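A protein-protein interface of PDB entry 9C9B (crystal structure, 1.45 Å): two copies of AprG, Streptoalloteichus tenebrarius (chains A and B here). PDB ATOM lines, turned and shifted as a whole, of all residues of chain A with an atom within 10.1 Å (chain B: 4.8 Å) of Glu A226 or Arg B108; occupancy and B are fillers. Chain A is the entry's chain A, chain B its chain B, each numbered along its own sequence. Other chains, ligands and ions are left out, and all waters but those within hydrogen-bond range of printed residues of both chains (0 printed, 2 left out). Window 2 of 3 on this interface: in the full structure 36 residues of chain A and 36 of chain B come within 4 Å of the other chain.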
ATOM      1  N   LEU A 151      16.254  19.807   0.944  1.00  0.00           N
ATOM      2  CA  LEU A 151      16.112  19.805  -0.510  1.00  0.00           C
ATOM      3  C   LEU A 151      16.375  21.188  -1.093  1.00  0.00           C
ATOM      4  O   LEU A 151      17.106  21.332  -2.078  1.00  0.00           O
ATOM      5  CB  LEU A 151      14.707  19.330  -0.871  1.00  0.00           C
ATOM      6  CG  LEU A 151      14.356  17.869  -1.075  1.00  0.00           C
ATOM      7  CD1 LEU A 151      12.909  17.678  -1.501  1.00  0.00           C
ATOM      8  CD2 LEU A 151      15.328  17.323  -2.128  1.00  0.00           C
ATOM      9  N   GLY A 154      20.069  21.681  -1.230  1.00  0.00           N
ATOM     10  CA  GLY A 154      20.838  20.734  -2.015  1.00  0.00           C
ATOM     11  C   GLY A 154      21.407  19.576  -1.233  1.00  0.00           C
ATOM     12  O   GLY A 154      22.252  18.840  -1.763  1.00  0.00           O
ATOM     13  N   VAL A 156      20.571  16.506  -0.450  1.00  0.00           N
ATOM     14  CA  VAL A 156      19.555  15.530  -0.842  1.00  0.00           C
ATOM     15  C   VAL A 156      19.644  14.256  -0.006  1.00  0.00           C
ATOM     16  O   VAL A 156      18.619  13.640   0.308  1.00  0.00           O
ATOM     17  CB  VAL A 156      19.610  15.270  -2.361  1.00  0.00           C
ATOM     18  CG1 VAL A 156      18.599  14.215  -2.765  1.00  0.00           C
ATOM     19  CG2 VAL A 156      19.351  16.563  -3.122  1.00  0.00           C
ATOM     20  N   ARG A 160      16.630  12.386   1.888  1.00  0.00           N
ATOM     21  CA  ARG A 160      16.258  10.986   1.725  1.00  0.00           C
ATOM     22  C   ARG A 160      16.166  10.286   3.073  1.00  0.00           C
ATOM     23  O   ARG A 160      15.262   9.477   3.303  1.00  0.00           O
ATOM     24  CB  ARG A 160      17.275  10.277   0.831  1.00  0.00           C
ATOM     25  CG  ARG A 160      17.165  10.608  -0.654  1.00  0.00           C
ATOM     26  CD  ARG A 160      18.206   9.772  -1.426  1.00  0.00           C
ATOM     27  NE  ARG A 160      18.188   9.954  -2.876  1.00  0.00           N
ATOM     28  CZ  ARG A 160      17.401   9.270  -3.708  1.00  0.00           C
ATOM     29  NH1 ARG A 160      17.465   9.487  -5.017  1.00  0.00           N
ATOM     30  NH2 ARG A 160      16.552   8.368  -3.238  1.00  0.00           N
ATOM     31  N   LEU A 218       7.342  14.814   1.070  1.00  0.00           N
ATOM     32  CA  LEU A 218       7.614  13.607   0.296  1.00  0.00           C
ATOM     33  C   LEU A 218       7.332  13.814  -1.186  1.00  0.00           C
ATOM     34  O   LEU A 218       8.036  13.263  -2.044  1.00  0.00           O
ATOM     35  CB  LEU A 218       6.776  12.450   0.834  1.00  0.00           C
ATOM     36  CG  LEU A 218       7.227  11.942   2.199  1.00  0.00           C
ATOM     37  CD1 LEU A 218       6.089  11.176   2.860  1.00  0.00           C
ATOM     38  CD2 LEU A 218       8.485  11.089   2.071  1.00  0.00           C
ATOM     39  N   THR A 219       6.296  14.587  -1.511  1.00  0.00           N
ATOM     40  CA  THR A 219       6.015  14.889  -2.909  1.00  0.00           C
ATOM     41  C   THR A 219       7.145  15.697  -3.531  1.00  0.00           C
ATOM     42  O   THR A 219       7.573  15.420  -4.657  1.00  0.00           O
ATOM     43  CB  THR A 219       4.679  15.622  -3.024  1.00  0.00           C
ATOM     44  OG1 THR A 219       3.649  14.841  -2.405  1.00  0.00           O
ATOM     45  CG2 THR A 219       4.333  15.826  -4.502  1.00  0.00           C
ATOM     46  N   ALA A 220       7.654  16.695  -2.803  1.00  0.00           N
ATOM     47  CA  ALA A 220       8.779  17.476  -3.308  1.00  0.00           C
ATOM     48  C   ALA A 220      10.021  16.609  -3.478  1.00  0.00           C
ATOM     49  O   ALA A 220      10.796  16.801  -4.424  1.00  0.00           O
ATOM     50  CB  ALA A 220       9.073  18.630  -2.356  1.00  0.00           C
ATOM     51  N   LEU A 221      10.235  15.658  -2.556  1.00  0.00           N
ATOM     52  CA  LEU A 221      11.368  14.754  -2.682  1.00  0.00           C
ATOM     53  C   LEU A 221      11.211  13.847  -3.894  1.00  0.00           C
ATOM     54  O   LEU A 221      12.186  13.579  -4.604  1.00  0.00           O
ATOM     55  CB  LEU A 221      11.553  13.946  -1.399  1.00  0.00           C
ATOM     56  CG  LEU A 221      12.730  12.966  -1.406  1.00  0.00           C
ATOM     57  CD1 LEU A 221      14.061  13.674  -1.577  1.00  0.00           C
ATOM     58  CD2 LEU A 221      12.720  12.162  -0.115  1.00  0.00           C
ATOM     59  N   TYR A 222       9.987  13.377  -4.152  1.00  0.00           N
ATOM     60  CA  TYR A 222       9.734  12.643  -5.385  1.00  0.00           C
ATOM     61  C   TYR A 222      10.039  13.504  -6.606  1.00  0.00           C
ATOM     62  O   TYR A 222      10.683  13.049  -7.559  1.00  0.00           O
ATOM     63  CB  TYR A 222       8.288  12.140  -5.423  1.00  0.00           C
ATOM     64  CG  TYR A 222       7.940  11.564  -6.773  1.00  0.00           C
ATOM     65  CD1 TYR A 222       8.504  10.369  -7.195  1.00  0.00           C
ATOM     66  CD2 TYR A 222       7.091  12.234  -7.637  1.00  0.00           C
ATOM     67  CE1 TYR A 222       8.214   9.840  -8.450  1.00  0.00           C
ATOM     68  CE2 TYR A 222       6.791  11.715  -8.889  1.00  0.00           C
ATOM     69  CZ  TYR A 222       7.363  10.521  -9.287  1.00  0.00           C
ATOM     70  OH  TYR A 222       7.063  10.010 -10.528  1.00  0.00           O
ATOM     71  N   GLU A 223       9.582  14.757  -6.606  1.00  0.00           N
ATOM     72  CA  GLU A 223       9.903  15.623  -7.733  1.00  0.00           C
ATOM     73  C   GLU A 223      11.411  15.715  -7.939  1.00  0.00           C
ATOM     74  O   GLU A 223      11.893  15.658  -9.076  1.00  0.00           O
ATOM     75  CB  GLU A 223       9.311  17.015  -7.515  1.00  0.00           C
ATOM     76  CG  GLU A 223       9.638  17.953  -8.642  1.00  0.00           C
ATOM     77  CD  GLU A 223       8.781  19.191  -8.643  1.00  0.00           C
ATOM     78  OE1 GLU A 223       8.810  19.927  -9.650  1.00  0.00           O
ATOM     79  OE2 GLU A 223       8.076  19.425  -7.638  1.00  0.00           O
ATOM     80  N   ALA A 224      12.174  15.797  -6.838  1.00  0.00           N
ATOM     81  CA  ALA A 224      13.618  15.986  -6.902  1.00  0.00           C
ATOM     82  C   ALA A 224      14.354  14.741  -7.382  1.00  0.00           C
ATOM     83  O   ALA A 224      15.417  14.860  -8.000  1.00  0.00           O
ATOM     84  CB  ALA A 224      14.141  16.361  -5.515  1.00  0.00           C
ATOM     85  N   THR A 225      13.823  13.548  -7.094  1.00  0.00           N
ATOM     86  CA  THR A 225      14.563  12.307  -7.297  1.00  0.00           C
ATOM     87  C   THR A 225      13.906  11.349  -8.267  1.00  0.00           C
ATOM     88  O   THR A 225      14.599  10.476  -8.806  1.00  0.00           O
ATOM     89  CB  THR A 225      14.692  11.528  -5.976  1.00  0.00           C
ATOM     90  OG1 THR A 225      13.380  11.159  -5.508  1.00  0.00           O
ATOM     91  CG2 THR A 225      15.431  12.325  -4.921  1.00  0.00           C
ATOM     92  N   GLU A 226      12.602  11.468  -8.477  1.00  0.00           N
ATOM     93  CA  GLU A 226      11.800  10.525  -9.250  1.00  0.00           C
ATOM     94  C   GLU A 226      11.831   9.111  -8.674  1.00  0.00           C
ATOM     95  O   GLU A 226      11.541   8.141  -9.381  1.00  0.00           O
ATOM     96  CB  GLU A 226      12.107  10.582 -10.752  1.00  0.00           C
ATOM     97  CG  GLU A 226      11.341  11.712 -11.436  1.00  0.00           C
ATOM     98  CD  GLU A 226      11.778  11.963 -12.863  1.00  0.00           C
ATOM     99  OE1 GLU A 226      12.998  12.091 -13.104  1.00  0.00           O
ATOM    100  OE2 GLU A 226      10.897  12.029 -13.744  1.00  0.00           O
ATOM    101  N   ASP A 227      12.148   8.984  -7.385  1.00  0.00           N
ATOM    102  CA  ASP A 227      12.111   7.704  -6.678  1.00  0.00           C
ATOM    103  C   ASP A 227      10.668   7.444  -6.250  1.00  0.00           C
ATOM    104  O   ASP A 227      10.136   8.125  -5.361  1.00  0.00           O
ATOM    105  CB  ASP A 227      13.046   7.753  -5.472  1.00  0.00           C
ATOM    106  CG  ASP A 227      13.199   6.411  -4.780  1.00  0.00           C
ATOM    107  OD1 ASP A 227      12.258   5.586  -4.816  1.00  0.00           O
ATOM    108  OD2 ASP A 227      14.278   6.178  -4.196  1.00  0.00           O
ATOM    109  N   ARG A 228      10.035   6.437  -6.859  1.00  0.00           N
ATOM    110  CA  ARG A 228       8.608   6.245  -6.647  1.00  0.00           C
ATOM    111  C   ARG A 228       8.267   5.836  -5.217  1.00  0.00           C
ATOM    112  O   ARG A 228       7.113   5.992  -4.806  1.00  0.00           O
ATOM    113  CB  ARG A 228       8.026   5.277  -7.684  1.00  0.00           C
ATOM    114  CG  ARG A 228       6.504   5.164  -7.631  1.00  0.00           C
ATOM    115  CD  ARG A 228       5.993   3.887  -8.268  1.00  0.00           C
ATOM    116  NE  ARG A 228       5.078   3.171  -7.385  1.00  0.00           N
ATOM    117  CZ  ARG A 228       4.941   1.848  -7.371  1.00  0.00           C
ATOM    118  NH1 ARG A 228       5.654   1.094  -8.199  1.00  0.00           N
ATOM    119  NH2 ARG A 228       4.089   1.277  -6.533  1.00  0.00           N
ATOM    120  N   ALA A 229       9.238   5.357  -4.432  1.00  0.00           N
ATOM    121  CA  ALA A 229       8.949   5.080  -3.027  1.00  0.00           C
ATOM    122  C   ALA A 229       8.418   6.326  -2.324  1.00  0.00           C
ATOM    123  O   ALA A 229       7.516   6.242  -1.481  1.00  0.00           O
ATOM    124  CB  ALA A 229      10.187   4.553  -2.308  1.00  0.00           C
ATOM    125  N   TYR A 230       8.941   7.497  -2.684  1.00  0.00           N
ATOM    126  CA  TYR A 230       8.499   8.717  -2.020  1.00  0.00           C
ATOM    127  C   TYR A 230       7.113   9.135  -2.492  1.00  0.00           C
ATOM    128  O   TYR A 230       6.305   9.633  -1.696  1.00  0.00           O
ATOM    129  CB  TYR A 230       9.518   9.831  -2.258  1.00  0.00           C
ATOM    130  CG  TYR A 230      10.919   9.445  -1.865  1.00  0.00           C
ATOM    131  CD1 TYR A 230      11.169   8.747  -0.690  1.00  0.00           C
ATOM    132  CD2 TYR A 230      11.992   9.764  -2.685  1.00  0.00           C
ATOM    133  CE1 TYR A 230      12.458   8.383  -0.334  1.00  0.00           C
ATOM    134  CE2 TYR A 230      13.283   9.404  -2.343  1.00  0.00           C
ATOM    135  CZ  TYR A 230      13.511   8.717  -1.173  1.00  0.00           C
ATOM    136  OH  TYR A 230      14.805   8.371  -0.856  1.00  0.00           O
ATOM    137  N   LEU A 231       6.837   8.977  -3.791  1.00  0.00           N
ATOM    138  CA  LEU A 231       5.497   9.228  -4.308  1.00  0.00           C
ATOM    139  C   LEU A 231       4.482   8.297  -3.662  1.00  0.00           C
ATOM    140  O   LEU A 231       3.372   8.720  -3.324  1.00  0.00           O
ATOM    141  CB  LEU A 231       5.476   9.069  -5.831  1.00  0.00           C
ATOM    142  CG  LEU A 231       4.114   9.247  -6.510  1.00  0.00           C
ATOM    143  CD1 LEU A 231       3.571  10.639  -6.246  1.00  0.00           C
ATOM    144  CD2 LEU A 231       4.222   8.984  -8.013  1.00  0.00           C
ATOM    145  N   ASP A 232       4.850   7.026  -3.474  1.00  0.00           N
ATOM    146  CA  ASP A 232       3.917   6.065  -2.888  1.00  0.00           C
ATOM    147  C   ASP A 232       3.556   6.448  -1.464  1.00  0.00           C
ATOM    148  O   ASP A 232       2.394   6.347  -1.063  1.00  0.00           O
ATOM    149  CB  ASP A 232       4.513   4.658  -2.891  1.00  0.00           C
ATOM    150  CG  ASP A 232       4.660   4.085  -4.287  1.00  0.00           C
ATOM    151  OD1 ASP A 232       4.037   4.620  -5.228  1.00  0.00           O
ATOM    152  OD2 ASP A 232       5.405   3.098  -4.440  1.00  0.00           O
ATOM    153  N   ARG A 267      -0.064  18.517 -10.197  1.00  0.00           N
ATOM    154  CA  ARG A 267       0.838  18.875 -11.286  1.00  0.00           C
ATOM    155  C   ARG A 267       1.672  17.681 -11.729  1.00  0.00           C
ATOM    156  O   ARG A 267       1.894  17.484 -12.928  1.00  0.00           O
ATOM    157  CB  ARG A 267       1.756  20.031 -10.894  1.00  0.00           C
ATOM    158  CG  ARG A 267       2.759  20.307 -11.987  1.00  0.00           C
ATOM    159  CD  ARG A 267       3.472  21.619 -11.834  1.00  0.00           C
ATOM    160  NE  ARG A 267       4.265  21.728 -10.615  1.00  0.00           N
ATOM    161  CZ  ARG A 267       5.482  21.218 -10.442  1.00  0.00           C
ATOM    162  NH1 ARG A 267       6.085  20.535 -11.404  1.00  0.00           N
ATOM    163  NH2 ARG A 267       6.106  21.413  -9.290  1.00  0.00           N
ATOM    164  N   LEU A 268       2.119  16.861 -10.779  1.00  0.00           N
ATOM    165  CA  LEU A 268       3.031  15.770 -11.113  1.00  0.00           C
ATOM    166  C   LEU A 268       2.311  14.561 -11.709  1.00  0.00           C
ATOM    167  O   LEU A 268       2.887  13.858 -12.548  1.00  0.00           O
ATOM    168  CB  LEU A 268       3.820  15.350  -9.875  1.00  0.00           C
ATOM    169  CG  LEU A 268       4.733  16.439  -9.311  1.00  0.00           C
ATOM    170  CD1 LEU A 268       5.461  15.899  -8.099  1.00  0.00           C
ATOM    171  CD2 LEU A 268       5.719  16.901 -10.360  1.00  0.00           C
ATOM    172  N   PHE B 104      12.526  20.868  -8.463  1.00  0.00           N
ATOM    173  CA  PHE B 104      13.794  20.243  -8.108  1.00  0.00           C
ATOM    174  C   PHE B 104      14.232  19.216  -9.130  1.00  0.00           C
ATOM    175  O   PHE B 104      15.432  18.948  -9.249  1.00  0.00           O
ATOM    176  CB  PHE B 104      13.695  19.584  -6.738  1.00  0.00           C
ATOM    177  CG  PHE B 104      13.519  20.562  -5.622  1.00  0.00           C
ATOM    178  CD1 PHE B 104      14.364  21.653  -5.501  1.00  0.00           C
ATOM    179  CD2 PHE B 104      12.495  20.402  -4.711  1.00  0.00           C
ATOM    180  CE1 PHE B 104      14.187  22.573  -4.466  1.00  0.00           C
ATOM    181  CE2 PHE B 104      12.316  21.312  -3.677  1.00  0.00           C
ATOM    182  CZ  PHE B 104      13.160  22.399  -3.558  1.00  0.00           C
ATOM    183  N   GLY B 105      13.287  18.601  -9.843  1.00  0.00           N
ATOM    184  CA  GLY B 105      13.687  17.679 -10.893  1.00  0.00           C
ATOM    185  C   GLY B 105      14.301  18.421 -12.062  1.00  0.00           C
ATOM    186  O   GLY B 105      15.357  18.036 -12.578  1.00  0.00           O
ATOM    187  N   LEU B 106      13.666  19.524 -12.465  1.00  0.00           N
ATOM    188  CA  LEU B 106      14.214  20.374 -13.512  1.00  0.00           C
ATOM    189  C   LEU B 106      15.592  20.902 -13.124  1.00  0.00           C
ATOM    190  O   LEU B 106      16.543  20.831 -13.912  1.00  0.00           O
ATOM    191  CB  LEU B 106      13.235  21.524 -13.782  1.00  0.00           C
ATOM    192  CG  LEU B 106      13.574  22.490 -14.923  1.00  0.00           C
ATOM    193  CD1 LEU B 106      13.851  21.747 -16.238  1.00  0.00           C
ATOM    194  CD2 LEU B 106      12.473  23.531 -15.105  1.00  0.00           C
ATOM    195  N   SER B 107      15.732  21.431 -11.903  1.00  0.00           N
ATOM    196  CA  SER B 107      17.017  21.996 -11.511  1.00  0.00           C
ATOM    197  C   SER B 107      18.102  20.925 -11.421  1.00  0.00           C
ATOM    198  O   SER B 107      19.233  21.159 -11.848  1.00  0.00           O
ATOM    199  CB  SER B 107      16.887  22.824 -10.230  1.00  0.00           C
ATOM    200  OG  SER B 107      16.689  22.001  -9.110  1.00  0.00           O
ATOM    201  N   ARG B 108      17.775  19.736 -10.894  1.00  0.00           N
ATOM    202  CA  ARG B 108      18.777  18.667 -10.840  1.00  0.00           C
ATOM    203  C   ARG B 108      19.229  18.265 -12.238  1.00  0.00           C
ATOM    204  O   ARG B 108      20.431  18.091 -12.492  1.00  0.00           O
ATOM    205  CB  ARG B 108      18.226  17.447 -10.099  1.00  0.00           C
ATOM    206  CG  ARG B 108      19.162  16.226 -10.170  1.00  0.00           C
ATOM    207  CD  ARG B 108      18.572  15.017  -9.451  1.00  0.00           C
ATOM    208  NE  ARG B 108      17.339  14.560 -10.088  1.00  0.00           N
ATOM    209  CZ  ARG B 108      17.293  13.815 -11.190  1.00  0.00           C
ATOM    210  NH1 ARG B 108      18.415  13.428 -11.783  1.00  0.00           N
ATOM    211  NH2 ARG B 108      16.125  13.445 -11.695  1.00  0.00           N
ATOM    212  N   LYS B 109      18.284  18.114 -13.158  1.00  0.00           N
ATOM    213  CA  LYS B 109      18.650  17.666 -14.497  1.00  0.00           C
ATOM    214  C   LYS B 109      19.460  18.730 -15.224  1.00  0.00           C
ATOM    215  O   LYS B 109      20.484  18.420 -15.846  1.00  0.00           O
ATOM    216  CB  LYS B 109      17.401  17.285 -15.282  1.00  0.00           C
ATOM    217  CG  LYS B 109      16.741  16.012 -14.747  1.00  0.00           C
ATOM    218  CD  LYS B 109      15.323  15.875 -15.264  1.00  0.00           C
ATOM    219  CE  LYS B 109      14.612  14.727 -14.566  1.00  0.00           C
ATOM    220  NZ  LYS B 109      13.173  14.680 -14.933  1.00  0.00           N
ATOM    221  N   LEU B 110      19.045  19.998 -15.117  1.00  0.00           N
ATOM    222  CA  LEU B 110      19.796  21.070 -15.759  1.00  0.00           C
ATOM    223  C   LEU B 110      21.198  21.197 -15.175  1.00  0.00           C
ATOM    224  O   LEU B 110      22.174  21.372 -15.916  1.00  0.00           O
ATOM    225  CB  LEU B 110      19.049  22.398 -15.603  1.00  0.00           C
ATOM    226  CG  LEU B 110      17.736  22.600 -16.352  1.00  0.00           C
ATOM    227  CD1 LEU B 110      17.030  23.837 -15.810  1.00  0.00           C
ATOM    228  CD2 LEU B 110      18.012  22.730 -17.849  1.00  0.00           C
ATOM    229  N   MET B 111      21.318  21.117 -13.846  1.00  0.00           N
ATOM    230  CA  MET B 111      22.611  21.336 -13.209  1.00  0.00           C
ATOM    231  C   MET B 111      23.544  20.169 -13.473  1.00  0.00           C
ATOM    232  O   MET B 111      24.757  20.358 -13.622  1.00  0.00           O
ATOM    233  CB  MET B 111      22.436  21.516 -11.699  1.00  0.00           C
ATOM    234  CG  MET B 111      23.722  21.928 -10.972  1.00  0.00           C
ATOM    235  SD  MET B 111      24.281  23.584 -11.425  1.00  0.00           S
ATOM    236  CE  MET B 111      26.069  23.401 -11.399  1.00  0.00           C
ATOM    237  N   SER B 112      22.996  18.956 -13.517  1.00  0.00           N
ATOM    238  CA  SER B 112      23.821  17.802 -13.848  1.00  0.00           C
ATOM    239  C   SER B 112      24.392  17.920 -15.252  1.00  0.00           C
ATOM    240  O   SER B 112      25.566  17.592 -15.479  1.00  0.00           O
ATOM    241  CB  SER B 112      23.007  16.524 -13.675  1.00  0.00           C
ATOM    242  OG  SER B 112      22.742  16.335 -12.294  1.00  0.00           O
ATOM    243  N   ARG B 155      25.654  22.882  -4.600  1.00  0.00           N
ATOM    244  CA  ARG B 155      26.874  22.200  -5.041  1.00  0.00           C
ATOM    245  C   ARG B 155      28.068  23.128  -4.810  1.00  0.00           C
ATOM    246  O   ARG B 155      28.688  23.651  -5.734  1.00  0.00           O
ATOM    247  CB  ARG B 155      26.742  21.771  -6.499  1.00  0.00           C
ATOM    248  CG  ARG B 155      25.447  21.027  -6.843  1.00  0.00           C
ATOM    249  CD  ARG B 155      25.625  20.099  -8.039  1.00  0.00           C
ATOM    250  NE  ARG B 155      24.351  19.638  -8.591  1.00  0.00           N
ATOM    251  CZ  ARG B 155      24.214  18.584  -9.395  1.00  0.00           C
ATOM    252  NH1 ARG B 155      25.269  17.867  -9.738  1.00  0.00           N
ATOM    253  NH2 ARG B 155      23.014  18.241  -9.848  1.00  0.00           N
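No position is printed for both chains.
O of Glu A223 lies close to N of Gly B105, at 3.3 Å. O of Ala A224 is in hydrogen-bond range of NE of Arg B108, at 2.9 Å. The side-chain carboxylate (OE1) of Glu A226 lies within salt-bridge range of the guanidinium group (NH2) of Arg B108. OE1 of Glu A226 is in salt-bridge range of NZ of Lys B109, 3.2 Å away.
Among the printed residues, merely in contact across the chains: Leu A151 with Phe B104, Ala A220 with Phe B104, Ala A224 with Phe B104 and Ala A224 with Gly B105.
Hydrophobic or aromatic side chains of chain A within 4 Å of the printed part of chain B: Ala A224. Of the 10 printed residues of chain B, 4 touch a printed residue of chain A. Printed residues of chain B that touch a printed residue of chain A: Phe B104, Gly B105, Arg B108 and Lys B109. Hydrophobic or aromatic side chains of chain B within 4 Å of the printed part of chain A: Phe B104. Along chain B the printed residues that touch a printed residue of chain A span positions 104 to 109. Among the printed residues, 8 pairs touch across the chains. Among the printed residues, Asp or Glu carboxylates within 4 Å of a Lys or Arg side-chain nitrogen of the other chain: Glu A226 with Arg B108 and Glu A226 with Lys B109.
Of the printed residues of chain B, Glu A226 touches Arg B108 (3.7 Å) and Lys B109 (3.2 Å). Of the printed residues of chain A, Arg B108 touches Ala A224 and Glu A226. Printed residues of chain A within 4 Å of Gly B105: Glu A223 and Ala A224. No residue of chain A comes within 4 Å of Ser B107. No residue of chain A comes within 4 Å of Ser B112. Printed residues of chain B within 4 Å of Ala A224: Phe B104 (3.5 Å), Gly B105 (3.9 Å) and Arg B108 (2.9 Å). Printed residues of chain B within 4 Å of Ala A220: Phe B104. The nearest printed residue of chain B that does not touch Glu A226 is Gly B105 (6.0 Å). The nearest printed residue of chain B that does not touch Ala A224 is Leu B106 (6.6 Å).
The guanidinium group of Arg A267 is in salt-bridge range of the side-chain carboxylate of Glu A223. O of Phe B104 lies within hydrogen-bond range of OG of Ser B107 (3.3 Å). The backbone carbonyl oxygen of Arg B108 lies within hydrogen-bond range of the side-chain hydroxyl of Ser B112 (2.9 Å).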
